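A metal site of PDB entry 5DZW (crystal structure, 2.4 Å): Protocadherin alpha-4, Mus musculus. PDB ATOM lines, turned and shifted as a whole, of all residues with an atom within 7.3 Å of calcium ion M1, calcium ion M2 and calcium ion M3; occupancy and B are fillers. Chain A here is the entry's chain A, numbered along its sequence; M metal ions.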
ATOM      1  N   GLU A 115      -8.495 -35.526  19.302  1.00  0.00           N
ATOM      2  CA  GLU A 115      -8.430 -35.609  20.763  1.00  0.00           C
ATOM      3  C   GLU A 115      -9.566 -34.809  21.405  1.00  0.00           C
ATOM      4  O   GLU A 115      -9.927 -35.045  22.558  1.00  0.00           O
ATOM      5  CB  GLU A 115      -7.077 -35.089  21.249  1.00  0.00           C
ATOM      6  CG  GLU A 115      -6.826 -35.247  22.739  1.00  0.00           C
ATOM      7  CD  GLU A 115      -5.602 -34.497  23.208  1.00  0.00           C
ATOM      8  OE1 GLU A 115      -4.904 -33.897  22.362  1.00  0.00           O
ATOM      9  OE2 GLU A 115      -5.337 -34.493  24.430  1.00  0.00           O
ATOM     10  N   LEU A 171      -9.865 -39.262  25.764  1.00  0.00           N
ATOM     11  CA  LEU A 171      -8.654 -39.596  25.015  1.00  0.00           C
ATOM     12  C   LEU A 171      -7.628 -38.468  25.090  1.00  0.00           C
ATOM     13  O   LEU A 171      -7.975 -37.291  25.008  1.00  0.00           O
ATOM     14  CB  LEU A 171      -9.001 -39.907  23.557  1.00  0.00           C
ATOM     15  CG  LEU A 171      -9.396 -38.786  22.591  1.00  0.00           C
ATOM     16  CD1 LEU A 171      -9.406 -39.304  21.163  1.00  0.00           C
ATOM     17  CD2 LEU A 171     -10.756 -38.174  22.937  1.00  0.00           C
ATOM     18  N   ASP A 172      -6.364 -38.838  25.244  1.00  0.00           N
ATOM     19  CA  ASP A 172      -5.284 -37.872  25.349  1.00  0.00           C
ATOM     20  C   ASP A 172      -4.108 -38.249  24.443  1.00  0.00           C
ATOM     21  O   ASP A 172      -3.499 -39.299  24.620  1.00  0.00           O
ATOM     22  CB  ASP A 172      -4.814 -37.746  26.802  1.00  0.00           C
ATOM     23  CG  ASP A 172      -3.698 -36.726  26.971  1.00  0.00           C
ATOM     24  OD1 ASP A 172      -4.019 -35.520  27.083  1.00  0.00           O
ATOM     25  OD2 ASP A 172      -2.519 -37.123  26.994  1.00  0.00           O
ATOM     26  N   ARG A 173      -3.802 -37.374  23.498  1.00  0.00           N
ATOM     27  CA  ARG A 173      -2.743 -37.600  22.528  1.00  0.00           C
ATOM     28  C   ARG A 173      -1.367 -37.770  23.192  1.00  0.00           C
ATOM     29  O   ARG A 173      -0.575 -38.613  22.769  1.00  0.00           O
ATOM     30  CB  ARG A 173      -2.710 -36.463  21.512  1.00  0.00           C
ATOM     31  CG  ARG A 173      -1.468 -36.401  20.645  1.00  0.00           C
ATOM     32  CD  ARG A 173      -0.588 -35.219  21.037  1.00  0.00           C
ATOM     33  NE  ARG A 173       0.477 -34.982  20.069  1.00  0.00           N
ATOM     34  CZ  ARG A 173       1.691 -35.522  20.153  1.00  0.00           C
ATOM     35  NH1 ARG A 173       2.606 -35.253  19.232  1.00  0.00           N
ATOM     36  NH2 ARG A 173       1.989 -36.331  21.157  1.00  0.00           N
ATOM     37  N   GLU A 174      -1.099 -36.973  24.213  1.00  0.00           N
ATOM     38  CA  GLU A 174       0.190 -36.994  24.887  1.00  0.00           C
ATOM     39  C   GLU A 174       0.432 -38.289  25.661  1.00  0.00           C
ATOM     40  O   GLU A 174       1.545 -38.792  25.714  1.00  0.00           O
ATOM     41  CB  GLU A 174       0.335 -35.792  25.832  1.00  0.00           C
ATOM     42  CG  GLU A 174       0.583 -34.466  25.134  1.00  0.00           C
ATOM     43  CD  GLU A 174      -0.637 -33.941  24.402  1.00  0.00           C
ATOM     44  OE1 GLU A 174      -1.761 -34.376  24.731  1.00  0.00           O
ATOM     45  OE2 GLU A 174      -0.469 -33.099  23.491  1.00  0.00           O
ATOM     46  N   GLU A 175      -0.636 -38.814  26.259  1.00  0.00           N
ATOM     47  CA  GLU A 175      -0.533 -40.058  27.020  1.00  0.00           C
ATOM     48  C   GLU A 175      -0.334 -41.261  26.095  1.00  0.00           C
ATOM     49  O   GLU A 175       0.624 -42.024  26.253  1.00  0.00           O
ATOM     50  CB  GLU A 175      -1.783 -40.259  27.882  1.00  0.00           C
ATOM     51  CG  GLU A 175      -1.772 -41.530  28.713  1.00  0.00           C
ATOM     52  CD  GLU A 175      -2.943 -41.625  29.666  1.00  0.00           C
ATOM     53  OE1 GLU A 175      -3.488 -40.557  30.037  1.00  0.00           O
ATOM     54  OE2 GLU A 175      -3.324 -42.745  30.048  1.00  0.00           O
ATOM     55  N   LEU A 204      -5.286 -37.261  17.017  1.00  0.00           N
ATOM     56  CA  LEU A 204      -4.755 -35.990  16.556  1.00  0.00           C
ATOM     57  C   LEU A 204      -4.485 -35.045  17.727  1.00  0.00           C
ATOM     58  O   LEU A 204      -5.146 -35.114  18.760  1.00  0.00           O
ATOM     59  CB  LEU A 204      -5.715 -35.346  15.555  1.00  0.00           C
ATOM     60  CG  LEU A 204      -6.150 -36.243  14.397  1.00  0.00           C
ATOM     61  CD1 LEU A 204      -7.146 -35.541  13.483  1.00  0.00           C
ATOM     62  CD2 LEU A 204      -4.940 -36.736  13.607  1.00  0.00           C
ATOM     63  N   ASP A 205      -3.498 -34.167  17.556  1.00  0.00           N
ATOM     64  CA  ASP A 205      -3.099 -33.256  18.632  1.00  0.00           C
ATOM     65  C   ASP A 205      -4.060 -32.076  18.774  1.00  0.00           C
ATOM     66  O   ASP A 205      -4.221 -31.280  17.845  1.00  0.00           O
ATOM     67  CB  ASP A 205      -1.681 -32.747  18.389  1.00  0.00           C
ATOM     68  CG  ASP A 205      -1.198 -31.815  19.490  1.00  0.00           C
ATOM     69  OD1 ASP A 205      -1.544 -32.050  20.662  1.00  0.00           O
ATOM     70  OD2 ASP A 205      -0.473 -30.848  19.177  1.00  0.00           O
ATOM     71  N   ALA A 206      -4.693 -31.977  19.930  1.00  0.00           N
ATOM     72  CA  ALA A 206      -5.565 -30.849  20.241  1.00  0.00           C
ATOM     73  C   ALA A 206      -4.813 -29.837  21.101  1.00  0.00           C
ATOM     74  O   ALA A 206      -3.860 -30.192  21.781  1.00  0.00           O
ATOM     75  CB  ALA A 206      -6.824 -31.320  20.932  1.00  0.00           C
ATOM     76  N   ASN A 207      -5.258 -28.594  21.071  1.00  0.00           N
ATOM     77  CA  ASN A 207      -4.623 -27.547  21.880  1.00  0.00           C
ATOM     78  C   ASN A 207      -5.285 -27.445  23.255  1.00  0.00           C
ATOM     79  O   ASN A 207      -5.958 -26.469  23.562  1.00  0.00           O
ATOM     80  CB  ASN A 207      -4.690 -26.197  21.166  1.00  0.00           C
ATOM     81  CG  ASN A 207      -3.807 -25.156  21.822  1.00  0.00           C
ATOM     82  OD1 ASN A 207      -2.818 -25.480  22.473  1.00  0.00           O
ATOM     83  ND2 ASN A 207      -4.176 -23.884  21.666  1.00  0.00           N
ATOM     84  N   ASP A 208      -5.087 -28.475  24.070  1.00  0.00           N
ATOM     85  CA  ASP A 208      -5.743 -28.552  25.368  1.00  0.00           C
ATOM     86  C   ASP A 208      -4.748 -28.533  26.529  1.00  0.00           C
ATOM     87  O   ASP A 208      -5.104 -28.828  27.670  1.00  0.00           O
ATOM     88  CB  ASP A 208      -6.615 -29.810  25.451  1.00  0.00           C
ATOM     89  CG  ASP A 208      -5.838 -31.079  25.161  1.00  0.00           C
ATOM     90  OD1 ASP A 208      -4.909 -31.031  24.329  1.00  0.00           O
ATOM     91  OD2 ASP A 208      -6.166 -32.124  25.768  1.00  0.00           O
ATOM     92  N   ASN A 209      -3.496 -28.182  26.238  1.00  0.00           N
ATOM     93  CA  ASN A 209      -2.483 -28.062  27.269  1.00  0.00           C
ATOM     94  C   ASN A 209      -1.784 -26.707  27.253  1.00  0.00           C
ATOM     95  O   ASN A 209      -1.263 -26.279  26.219  1.00  0.00           O
ATOM     96  CB  ASN A 209      -1.443 -29.175  27.142  1.00  0.00           C
ATOM     97  CG  ASN A 209      -1.888 -30.473  27.800  1.00  0.00           C
ATOM     98  OD1 ASN A 209      -3.076 -30.791  27.809  1.00  0.00           O
ATOM     99  ND2 ASN A 209      -0.935 -31.206  28.357  1.00  0.00           N
ATOM    100  N   ALA A 210      -1.790 -26.031  28.396  1.00  0.00           N
ATOM    101  CA  ALA A 210      -1.152 -24.722  28.527  1.00  0.00           C
ATOM    102  C   ALA A 210       0.341 -24.879  28.817  1.00  0.00           C
ATOM    103  O   ALA A 210       0.762 -25.860  29.429  1.00  0.00           O
ATOM    104  CB  ALA A 210      -1.830 -23.924  29.630  1.00  0.00           C
ATOM    105  N   PRO A 211       1.153 -23.900  28.371  1.00  0.00           N
ATOM    106  CA  PRO A 211       2.582 -23.910  28.655  1.00  0.00           C
ATOM    107  C   PRO A 211       2.883 -23.793  30.144  1.00  0.00           C
ATOM    108  O   PRO A 211       2.095 -23.192  30.880  1.00  0.00           O
ATOM    109  CB  PRO A 211       3.101 -22.685  27.891  1.00  0.00           C
ATOM    110  CG  PRO A 211       1.909 -21.824  27.673  1.00  0.00           C
ATOM    111  CD  PRO A 211       0.760 -22.773  27.512  1.00  0.00           C
ATOM    112  N   ASP A 239       5.698 -27.009  26.841  1.00  0.00           N
ATOM    113  CA  ASP A 239       4.317 -27.323  26.504  1.00  0.00           C
ATOM    114  C   ASP A 239       4.223 -28.685  25.819  1.00  0.00           C
ATOM    115  O   ASP A 239       5.027 -29.006  24.945  1.00  0.00           O
ATOM    116  CB  ASP A 239       3.722 -26.224  25.616  1.00  0.00           C
ATOM    117  CG  ASP A 239       2.226 -26.375  25.414  1.00  0.00           C
ATOM    118  OD1 ASP A 239       1.595 -27.156  26.168  1.00  0.00           O
ATOM    119  OD2 ASP A 239       1.683 -25.713  24.514  1.00  0.00           O
ATOM    120  N   LEU A 240       3.225 -29.474  26.222  1.00  0.00           N
ATOM    121  CA  LEU A 240       3.124 -30.856  25.775  1.00  0.00           C
ATOM    122  C   LEU A 240       2.579 -31.001  24.354  1.00  0.00           C
ATOM    123  O   LEU A 240       2.815 -32.010  23.700  1.00  0.00           O
ATOM    124  CB  LEU A 240       2.249 -31.650  26.747  1.00  0.00           C
ATOM    125  CG  LEU A 240       2.839 -31.851  28.138  1.00  0.00           C
ATOM    126  CD1 LEU A 240       1.933 -32.720  28.997  1.00  0.00           C
ATOM    127  CD2 LEU A 240       4.233 -32.466  28.045  1.00  0.00           C
ATOM    128  N   ASP A 241       1.864 -29.988  23.879  1.00  0.00           N
ATOM    129  CA  ASP A 241       1.316 -30.030  22.525  1.00  0.00           C
ATOM    130  C   ASP A 241       2.406 -29.834  21.478  1.00  0.00           C
ATOM    131  O   ASP A 241       3.518 -29.406  21.801  1.00  0.00           O
ATOM    132  CB  ASP A 241       0.214 -28.979  22.356  1.00  0.00           C
ATOM    133  CG  ASP A 241      -0.942 -29.185  23.306  1.00  0.00           C
ATOM    134  OD1 ASP A 241      -0.939 -30.194  24.039  1.00  0.00           O
ATOM    135  OD2 ASP A 241      -1.867 -28.350  23.311  1.00  0.00           O
ATOM    136  N   GLU A 242       2.086 -30.150  20.231  1.00  0.00           N
ATOM    137  CA  GLU A 242       3.066 -30.073  19.147  1.00  0.00           C
ATOM    138  C   GLU A 242       2.658 -29.055  18.082  1.00  0.00           C
ATOM    139  O   GLU A 242       1.524 -28.584  18.063  1.00  0.00           O
ATOM    140  CB  GLU A 242       3.258 -31.449  18.511  1.00  0.00           C
ATOM    141  N   VAL A 244       2.331 -25.565  16.114  1.00  0.00           N
ATOM    142  CA  VAL A 244       2.110 -24.204  16.562  1.00  0.00           C
ATOM    143  C   VAL A 244       1.439 -24.195  17.936  1.00  0.00           C
ATOM    144  O   VAL A 244       1.457 -23.193  18.643  1.00  0.00           O
ATOM    145  CB  VAL A 244       1.248 -23.402  15.568  1.00  0.00           C
ATOM    146  CG1 VAL A 244       1.970 -23.237  14.242  1.00  0.00           C
ATOM    147  CG2 VAL A 244      -0.108 -24.074  15.362  1.00  0.00           C
ATOM    148  N   ASN A 245       0.841 -25.331  18.305  1.00  0.00           N
ATOM    149  CA  ASN A 245       0.232 -25.479  19.614  1.00  0.00           C
ATOM    150  C   ASN A 245       1.283 -25.722  20.689  1.00  0.00           C
ATOM    151  O   ASN A 245       0.980 -25.709  21.878  1.00  0.00           O
ATOM    152  CB  ASN A 245      -0.785 -26.620  19.610  1.00  0.00           C
ATOM    153  CG  ASN A 245      -1.937 -26.372  18.649  1.00  0.00           C
ATOM    154  OD1 ASN A 245      -1.943 -25.385  17.924  1.00  0.00           O
ATOM    155  ND2 ASN A 245      -2.898 -27.279  18.646  1.00  0.00           N
ATOM    156  N   GLY A 246       2.519 -25.929  20.252  1.00  0.00           N
ATOM    157  CA  GLY A 246       3.622 -26.183  21.163  1.00  0.00           C
ATOM    158  C   GLY A 246       4.577 -25.008  21.302  1.00  0.00           C
ATOM    159  O   GLY A 246       5.183 -24.807  22.354  1.00  0.00           O
ATOM    160  N   ASP A 247       4.721 -24.227  20.226  1.00  0.00           N
ATOM    161  CA  ASP A 247       5.613 -23.068  20.239  1.00  0.00           C
ATOM    162  C   ASP A 247       5.096 -21.980  21.169  1.00  0.00           C
ATOM    163  O   ASP A 247       3.913 -21.652  21.150  1.00  0.00           O
ATOM    164  CB  ASP A 247       5.789 -22.517  18.821  1.00  0.00           C
ATOM    165  CG  ASP A 247       6.640 -23.412  17.944  1.00  0.00           C
ATOM    166  OD1 ASP A 247       6.565 -24.650  18.099  1.00  0.00           O
ATOM    167  OD2 ASP A 247       7.383 -22.884  17.096  1.00  0.00           O
ATOM    168  N   ILE A 248       5.997 -21.423  21.984  1.00  0.00           N
ATOM    169  CA  ILE A 248       5.609 -20.456  23.004  1.00  0.00           C
ATOM    170  C   ILE A 248       6.221 -19.075  22.777  1.00  0.00           C
ATOM    171  O   ILE A 248       7.421 -18.944  22.548  1.00  0.00           O
ATOM    172  CB  ILE A 248       6.023 -20.950  24.405  1.00  0.00           C
ATOM    173  CG1 ILE A 248       5.584 -22.402  24.620  1.00  0.00           C
ATOM    174  CG2 ILE A 248       5.439 -20.047  25.490  1.00  0.00           C
ATOM    175  CD1 ILE A 248       6.100 -23.012  25.900  1.00  0.00           C
ATOM    176  N   ASP A 295       0.988 -19.888  23.804  1.00  0.00           N
ATOM    177  CA  ASP A 295       1.242 -20.698  22.614  1.00  0.00           C
ATOM    178  C   ASP A 295       0.633 -20.065  21.375  1.00  0.00           C
ATOM    179  O   ASP A 295      -0.002 -19.011  21.444  1.00  0.00           O
ATOM    180  CB  ASP A 295       0.713 -22.130  22.805  1.00  0.00           C
ATOM    181  CG  ASP A 295      -0.673 -22.168  23.411  1.00  0.00           C
ATOM    182  OD1 ASP A 295      -1.486 -21.269  23.112  1.00  0.00           O
ATOM    183  OD2 ASP A 295      -0.962 -23.100  24.185  1.00  0.00           O
ATOM    184  N   LYS A 296       0.821 -20.702  20.220  1.00  0.00           N
ATOM    185  CA  LYS A 296       0.386 -20.136  18.947  1.00  0.00           C
ATOM    186  C   LYS A 296      -0.696 -20.973  18.278  1.00  0.00           C
ATOM    187  O   LYS A 296      -0.668 -21.173  17.064  1.00  0.00           O
ATOM    188  CB  LYS A 296       1.590 -19.983  18.009  1.00  0.00           C
ATOM    189  CG  LYS A 296       2.740 -19.177  18.585  1.00  0.00           C
ATOM    190  CD  LYS A 296       3.916 -19.124  17.620  1.00  0.00           C
ATOM    191  N   GLY A 297      -1.651 -21.456  19.065  1.00  0.00           N
ATOM    192  CA  GLY A 297      -2.744 -22.244  18.538  1.00  0.00           C
ATOM    193  C   GLY A 297      -3.916 -21.384  18.124  1.00  0.00           C
ATOM    194  O   GLY A 297      -3.888 -20.160  18.283  1.00  0.00           O
ATOM    195  N   LEU A 299      -6.981 -21.475  19.469  1.00  0.00           N
ATOM    196  CA  LEU A 299      -7.413 -20.970  20.763  1.00  0.00           C
ATOM    197  C   LEU A 299      -6.232 -21.000  21.716  1.00  0.00           C
ATOM    198  O   LEU A 299      -5.946 -22.040  22.320  1.00  0.00           O
ATOM    199  CB  LEU A 299      -8.582 -21.783  21.318  1.00  0.00           C
ATOM    200  CG  LEU A 299      -9.128 -21.318  22.665  1.00  0.00           C
ATOM    201  CD1 LEU A 299      -9.512 -19.848  22.607  1.00  0.00           C
ATOM    202  CD2 LEU A 299     -10.302 -22.172  23.101  1.00  0.00           C
ATOM    203  N   PRO A 300      -5.528 -19.868  21.847  1.00  0.00           N
ATOM    204  CA  PRO A 300      -4.289 -19.771  22.629  1.00  0.00           C
ATOM    205  C   PRO A 300      -4.479 -20.069  24.105  1.00  0.00           C
ATOM    206  O   PRO A 300      -5.473 -19.636  24.706  1.00  0.00           O
ATOM    207  CB  PRO A 300      -3.861 -18.318  22.422  1.00  0.00           C
ATOM    208  CG  PRO A 300      -4.554 -17.873  21.175  1.00  0.00           C
ATOM    209  CD  PRO A 300      -5.863 -18.591  21.186  1.00  0.00           C
ATOM    210  N   LEU A 301      -3.535 -20.801  24.685  1.00  0.00           N
ATOM    211  CA  LEU A 301      -3.503 -21.023  26.129  1.00  0.00           C
ATOM    212  C   LEU A 301      -2.288 -20.317  26.730  1.00  0.00           C
ATOM    213  O   LEU A 301      -1.224 -20.250  26.108  1.00  0.00           O
ATOM    214  CB  LEU A 301      -3.457 -22.517  26.446  1.00  0.00           C
ATOM    215  CG  LEU A 301      -4.727 -23.309  26.121  1.00  0.00           C
ATOM    216  CD1 LEU A 301      -4.606 -24.743  26.612  1.00  0.00           C
ATOM    217  CD2 LEU A 301      -5.949 -22.629  26.724  1.00  0.00           C
HETATM  218 CA    CA M   1      -0.601 -25.834  23.907  1.00  0.00          CA
HETATM  219 CA    CA M   2      -2.604 -31.871  22.885  1.00  0.00          CA
HETATM  220 CA    CA M   3      -3.659 -33.007  25.400  1.00  0.00          CA
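OE1 of Glu 115 is in hydrogen-bond range of N of Ala 206, at 3.1 Å.
N of Glu 174 is in hydrogen-bond range of OD2 of Asp 172, at 3.1 Å.
The side-chain carboxylate (OE2) of Glu 115 sits close to the backbone NH (N) of Arg 173 (3.4 Å).
The backbone carbonyl oxygen of Leu 204 lies close to the backbone NH of Glu 115.
The side-chain carboxylate (OD1) of Asp 205 lies close to the guanidinium group (NE) of Arg 173, 3.6 Å away.
OD2 of Asp 205 lies within hydrogen-bond range of N of Glu 242 (2.9 Å).
OD1 of Asp 295 sits at hydrogen-bond distance from N of Leu 301 (2.6 Å).
The backbone NH of Glu 175 is in hydrogen-bond range of the side-chain carboxylate of Asp 172, 2.6 Å away.
Six residues have an atom within 4 Å of calcium ion M1: Asn 207, Asn 209, Asp 239, Asp 241, Asn 245 and Asp 295.
The nearest printed residue that does not touch calcium ion M1 is Ala 210 (4.6 Å).
Along chain A the residues within 4 Å of calcium ion M2 span positions 115 to 241.
Of the 29 residues printed, 5 come within 4 Å of calcium ion M3.
The nearest printed residue that does not touch calcium ion M3 is Asp 241 (4.1 Å).
Calcium ion M1 is bound by OD2 of Asp 239 (2.4 Å), O of Asn 209 (2.4 Å), O of Asn 245 (2.6 Å), OD1 of Asn 207 (2.7 Å), OD2 of Asp 295 (2.8 Å) and OD2 of Asp 241 (2.9 Å).
Calcium ion M2 is bound by the backbone carbonyl oxygen (O) of Ala 206 (2.4 Å), the side-chain carboxylate (OD1) of Asp 205 (2.5 Å), the side-chain carboxylate (OE2) of Glu 174 (2.5 Å), the side-chain carboxylate (OD1) of Asp 241 (2.6 Å) and the side-chain carboxylate (OD1) of Asp 208 (2.8 Å).
Calcium ion M2 has five donor atoms within binding distance.
Slightly farther from calcium ion M2 lies the side-chain carboxylate (OE1) of Glu 115 (3.1 Å).
Calcium ion M3 is bound by OE1 of Glu 174 (2.4 Å), OE2 of Glu 115 (2.4 Å), OD1 of Asp 208 (2.6 Å) and OD2 of Asp 208 (2.7 Å).
Calcium ion M3 has four donor atoms within binding distance.
Slightly farther from calcium ion M3 lies OD1 of Asp 172 (3.0 Å).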
